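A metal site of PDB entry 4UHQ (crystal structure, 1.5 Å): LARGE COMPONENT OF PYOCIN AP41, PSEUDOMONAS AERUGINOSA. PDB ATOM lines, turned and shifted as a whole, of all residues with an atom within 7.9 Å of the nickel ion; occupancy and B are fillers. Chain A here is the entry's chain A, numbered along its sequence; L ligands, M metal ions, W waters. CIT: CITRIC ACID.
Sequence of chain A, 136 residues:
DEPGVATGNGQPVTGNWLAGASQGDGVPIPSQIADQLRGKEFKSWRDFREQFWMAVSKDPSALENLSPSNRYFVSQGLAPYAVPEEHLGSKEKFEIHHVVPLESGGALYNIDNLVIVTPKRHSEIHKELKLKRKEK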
ATOM      1  N   GLU A  95       8.037  20.762  32.281  1.00  0.00           N
ATOM      2  CA  GLU A  95       9.089  21.742  32.529  1.00  0.00           C
ATOM      3  C   GLU A  95       9.323  22.608  31.330  1.00  0.00           C
ATOM      4  O   GLU A  95       9.153  22.164  30.197  1.00  0.00           O
ATOM      5  CB  GLU A  95      10.420  20.991  32.901  1.00  0.00           C
ATOM      6  CG  GLU A  95      10.244  20.328  34.294  1.00  0.00           C
ATOM      7  CD  GLU A  95      11.412  19.519  34.756  1.00  0.00           C
ATOM      8  OE1 GLU A  95      12.358  19.330  33.963  1.00  0.00           O
ATOM      9  OE2 GLU A  95      11.356  19.048  35.922  1.00  0.00           O
ATOM     10  N   ILE A  96       9.739  23.850  31.572  1.00  0.00           N
ATOM     11  CA  ILE A  96      10.145  24.754  30.512  1.00  0.00           C
ATOM     12  C   ILE A  96      11.671  24.683  30.411  1.00  0.00           C
ATOM     13  O   ILE A  96      12.373  25.012  31.385  1.00  0.00           O
ATOM     14  CB  ILE A  96       9.696  26.178  30.831  1.00  0.00           C
ATOM     15  CG1 ILE A  96       8.188  26.239  31.053  1.00  0.00           C
ATOM     16  CG2 ILE A  96      10.102  27.103  29.646  1.00  0.00           C
ATOM     17  CD1 ILE A  96       7.749  27.589  31.648  1.00  0.00           C
ATOM     18  N   HIS A  97      12.176  24.155  29.302  1.00  0.00           N
ATOM     19  CA  HIS A  97      13.625  24.005  29.110  1.00  0.00           C
ATOM     20  C   HIS A  97      14.145  25.078  28.165  1.00  0.00           C
ATOM     21  O   HIS A  97      13.508  25.449  27.160  1.00  0.00           O
ATOM     22  CB  HIS A  97      13.910  22.580  28.579  1.00  0.00           C
ATOM     23  CG  HIS A  97      15.201  22.396  27.836  1.00  0.00           C
ATOM     24  ND1 HIS A  97      16.467  22.351  28.437  1.00  0.00           N
ATOM     25  CD2 HIS A  97      15.419  22.125  26.517  1.00  0.00           C
ATOM     26  CE1 HIS A  97      17.380  22.104  27.517  1.00  0.00           C
ATOM     27  NE2 HIS A  97      16.773  21.965  26.340  1.00  0.00           N
ATOM     28  N   HIS A  98      15.306  25.621  28.523  1.00  0.00           N
ATOM     29  CA  HIS A  98      16.003  26.567  27.673  1.00  0.00           C
ATOM     30  C   HIS A  98      16.837  25.798  26.658  1.00  0.00           C
ATOM     31  O   HIS A  98      17.770  25.084  26.986  1.00  0.00           O
ATOM     32  CB  HIS A  98      16.893  27.483  28.551  1.00  0.00           C
ATOM     33  CG  HIS A  98      16.080  28.436  29.367  1.00  0.00           C
ATOM     34  ND1 HIS A  98      15.569  28.130  30.619  1.00  0.00           N
ATOM     35  CD2 HIS A  98      15.670  29.699  29.088  1.00  0.00           C
ATOM     36  CE1 HIS A  98      14.851  29.157  31.058  1.00  0.00           C
ATOM     37  NE2 HIS A  98      14.896  30.122  30.144  1.00  0.00           N
ATOM     38  N   VAL A  99      16.458  25.941  25.381  1.00  0.00           N
ATOM     39  CA  VAL A  99      17.001  25.146  24.286  1.00  0.00           C
ATOM     40  C   VAL A  99      18.505  25.316  24.177  1.00  0.00           C
ATOM     41  O   VAL A  99      19.236  24.326  24.079  1.00  0.00           O
ATOM     42  CB  VAL A  99      16.319  25.549  22.970  1.00  0.00           C
ATOM     43  CG1 VAL A  99      16.926  24.815  21.798  1.00  0.00           C
ATOM     44  CG2 VAL A  99      14.820  25.190  23.015  1.00  0.00           C
ATOM     45  N   VAL A 100      18.960  26.571  24.171  1.00  0.00           N
ATOM     46  CA  VAL A 100      20.366  26.881  24.472  1.00  0.00           C
ATOM     47  C   VAL A 100      20.380  27.107  25.979  1.00  0.00           C
ATOM     48  O   VAL A 100      19.741  28.036  26.495  1.00  0.00           O
ATOM     49  CB  VAL A 100      20.839  28.132  23.751  1.00  0.00           C
ATOM     50  CG1 VAL A 100      22.307  28.432  24.161  1.00  0.00           C
ATOM     51  CG2 VAL A 100      20.709  27.955  22.242  1.00  0.00           C
ATOM     52  N   PRO A 101      21.023  26.225  26.719  1.00  0.00           N
ATOM     53  CA  PRO A 101      20.947  26.359  28.161  1.00  0.00           C
ATOM     54  C   PRO A 101      21.481  27.676  28.701  1.00  0.00           C
ATOM     55  O   PRO A 101      22.347  28.332  28.108  1.00  0.00           O
ATOM     56  CB  PRO A 101      21.811  25.194  28.661  1.00  0.00           C
ATOM     57  CG  PRO A 101      21.614  24.153  27.567  1.00  0.00           C
ATOM     58  CD  PRO A 101      21.659  24.944  26.302  1.00  0.00           C
ATOM     59  N   LEU A 102      20.926  28.081  29.837  1.00  0.00           N
ATOM     60  CA  LEU A 102      21.417  29.314  30.474  1.00  0.00           C
ATOM     61  C   LEU A 102      22.898  29.249  30.727  1.00  0.00           C
ATOM     62  O   LEU A 102      23.644  30.203  30.571  1.00  0.00           O
ATOM     63  CB  LEU A 102      20.632  29.562  31.773  1.00  0.00           C
ATOM     64  CG  LEU A 102      19.111  29.580  31.610  1.00  0.00           C
ATOM     65  CD1 LEU A 102      18.405  29.692  32.981  1.00  0.00           C
ATOM     66  CD2 LEU A 102      18.767  30.758  30.771  1.00  0.00           C
ATOM     67  N   GLU A 103      23.364  28.049  31.072  1.00  0.00           N
ATOM     68  CA  GLU A 103      24.750  27.859  31.363  1.00  0.00           C
ATOM     69  C   GLU A 103      25.658  27.853  30.110  1.00  0.00           C
ATOM     70  O   GLU A 103      26.868  27.799  30.197  1.00  0.00           O
ATOM     71  CB  GLU A 103      24.926  26.540  32.159  1.00  0.00           C
ATOM     72  CG  GLU A 103      24.394  25.300  31.425  1.00  0.00           C
ATOM     73  CD  GLU A 103      24.735  23.982  32.136  1.00  0.00           C
ATOM     74  OE1 GLU A 103      25.132  24.028  33.323  1.00  0.00           O
ATOM     75  OE2 GLU A 103      24.602  22.917  31.503  1.00  0.00           O
ATOM     76  N   VAL A 115      11.295  25.414  25.189  1.00  0.00           N
ATOM     77  CA  VAL A 115      10.393  24.324  24.802  1.00  0.00           C
ATOM     78  C   VAL A 115       9.752  23.766  26.050  1.00  0.00           C
ATOM     79  O   VAL A 115      10.236  23.990  27.178  1.00  0.00           O
ATOM     80  CB  VAL A 115      11.119  23.187  24.052  1.00  0.00           C
ATOM     81  CG1 VAL A 115      11.571  23.646  22.666  1.00  0.00           C
ATOM     82  CG2 VAL A 115      12.340  22.661  24.892  1.00  0.00           C
ATOM     83  N   VAL A 117       9.025  20.216  27.944  1.00  0.00           N
ATOM     84  CA  VAL A 117       9.527  18.837  28.013  1.00  0.00           C
ATOM     85  C   VAL A 117       9.030  18.187  29.279  1.00  0.00           C
ATOM     86  O   VAL A 117       8.684  18.864  30.268  1.00  0.00           O
ATOM     87  CB  VAL A 117      11.073  18.781  28.003  1.00  0.00           C
ATOM     88  CG1 VAL A 117      11.602  19.027  26.585  1.00  0.00           C
ATOM     89  CG2 VAL A 117      11.632  19.841  29.004  1.00  0.00           C
ATOM     90  N   HIS A 122      13.618  16.136  29.746  1.00  0.00           N
ATOM     91  CA  HIS A 122      14.553  17.247  30.008  1.00  0.00           C
ATOM     92  C   HIS A 122      15.911  16.727  30.493  1.00  0.00           C
ATOM     93  O   HIS A 122      16.984  17.198  30.064  1.00  0.00           O
ATOM     94  CB  HIS A 122      13.927  18.152  31.075  1.00  0.00           C
ATOM     95  CG  HIS A 122      14.575  19.494  31.210  1.00  0.00           C
ATOM     96  ND1 HIS A 122      14.190  20.387  32.195  1.00  0.00           N
ATOM     97  CD2 HIS A 122      15.526  20.123  30.493  1.00  0.00           C
ATOM     98  CE1 HIS A 122      14.920  21.485  32.105  1.00  0.00           C
ATOM     99  NE2 HIS A 122      15.764  21.345  31.103  1.00  0.00           N
ATOM    100  N   SER A 123      15.897  15.767  31.400  1.00  0.00           N
ATOM    101  CA  SER A 123      17.140  15.171  31.871  1.00  0.00           C
ATOM    102  C   SER A 123      17.914  14.498  30.740  1.00  0.00           C
ATOM    103  O   SER A 123      19.171  14.678  30.646  1.00  0.00           O
ATOM    104  CB  SER A 123      16.821  14.197  32.992  1.00  0.00           C
ATOM    105  OG  SER A 123      17.987  13.558  33.478  1.00  0.00           O
ATOM    106  N   ILE A 125      17.801  15.238  27.616  1.00  0.00           N
ATOM    107  CA  ILE A 125      18.361  16.249  26.700  1.00  0.00           C
ATOM    108  C   ILE A 125      19.667  16.796  27.258  1.00  0.00           C
ATOM    109  O   ILE A 125      20.653  16.922  26.530  1.00  0.00           O
ATOM    110  CB  ILE A 125      17.349  17.382  26.481  1.00  0.00           C
ATOM    111  CG1 ILE A 125      16.219  16.875  25.597  1.00  0.00           C
ATOM    112  CG2 ILE A 125      18.019  18.647  25.906  1.00  0.00           C
ATOM    113  CD1 ILE A 125      15.017  17.872  25.534  1.00  0.00           C
ATOM    114  N   HIS A 126      19.720  17.047  28.554  1.00  0.00           N
ATOM    115  CA  HIS A 126      20.947  17.565  29.125  1.00  0.00           C
ATOM    116  C   HIS A 126      22.066  16.529  29.128  1.00  0.00           C
ATOM    117  O   HIS A 126      23.217  16.894  28.885  1.00  0.00           O
ATOM    118  CB  HIS A 126      20.691  18.120  30.508  1.00  0.00           C
ATOM    119  CG  HIS A 126      20.068  19.475  30.442  1.00  0.00           C
ATOM    120  ND1 HIS A 126      20.808  20.597  30.178  1.00  0.00           N
ATOM    121  CD2 HIS A 126      18.774  19.874  30.520  1.00  0.00           C
ATOM    122  CE1 HIS A 126      20.003  21.634  30.080  1.00  0.00           C
ATOM    123  NE2 HIS A 126      18.759  21.233  30.304  1.00  0.00           N
ATOM    124  N   LEU A 129      23.302  16.620  25.593  1.00  0.00           N
ATOM    125  CA  LEU A 129      24.113  17.795  25.283  1.00  0.00           C
ATOM    126  C   LEU A 129      25.503  17.630  25.827  1.00  0.00           C
ATOM    127  O   LEU A 129      26.502  18.043  25.219  1.00  0.00           O
ATOM    128  CB  LEU A 129      23.470  19.075  25.881  1.00  0.00           C
ATOM    129  CG  LEU A 129      22.180  19.527  25.199  1.00  0.00           C
ATOM    130  CD1 LEU A 129      21.533  20.679  26.002  1.00  0.00           C
ATOM    131  CD2 LEU A 129      22.547  19.997  23.807  1.00  0.00           C
HETATM  132  C1  CIT L   1      19.618  25.902  32.132  1.00  0.00           C
HETATM  133  O1  CIT L   1      20.865  26.194  32.310  1.00  0.00           O
HETATM  134  O2  CIT L   1      19.169  26.034  30.999  1.00  0.00           O
HETATM  135  C2  CIT L   1      18.814  25.365  33.290  1.00  0.00           C
HETATM  136  C3  CIT L   1      17.655  24.420  32.913  1.00  0.00           C
HETATM  137  O7  CIT L   1      18.191  23.273  32.280  1.00  0.00           O
HETATM  138  C4  CIT L   1      16.923  24.000  34.195  1.00  0.00           C
HETATM  139  C5  CIT L   1      17.764  23.058  35.007  1.00  0.00           C
HETATM  140  O3  CIT L   1      18.529  22.226  34.483  1.00  0.00           O
HETATM  141  O4  CIT L   1      17.682  23.186  36.237  1.00  0.00           O
HETATM  142  C6  CIT L   1      16.603  25.008  31.999  1.00  0.00           C
HETATM  143  O5  CIT L   1      16.186  26.161  32.316  1.00  0.00           O
HETATM  144  O6  CIT L   1      16.240  24.406  30.964  1.00  0.00           O
HETATM  145 NI    NI M   1      17.200  22.659  30.366  1.00  0.00          NI
HETATM  146  O   HOH W   1      18.547  24.036  29.393  1.00  0.00           O
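A ring nitrogen (ND1) of His 122 lies within hydrogen-bond range of the side-chain carboxylate (OE1) of Glu 95 (2.8 Å).
N of His 97 is in hydrogen-bond range of O of Val 115 (2.9 Å).
His 98 touches the nickel ion (N to NI, 3.97 Å).
Of the 16 residues printed, 4 come within 4 Å of the nickel ion.
The nickel ion is bound by O6 of the ligand (2.1 Å), NE2 of His 122 (2.1 Å), ND1 of His 97 (2.1 Å), NE2 of His 126 (2.1 Å), water W1 (2.2 Å) and O7 of the ligand (2.2 Å).
The nickel ion has six donor atoms within binding distance.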
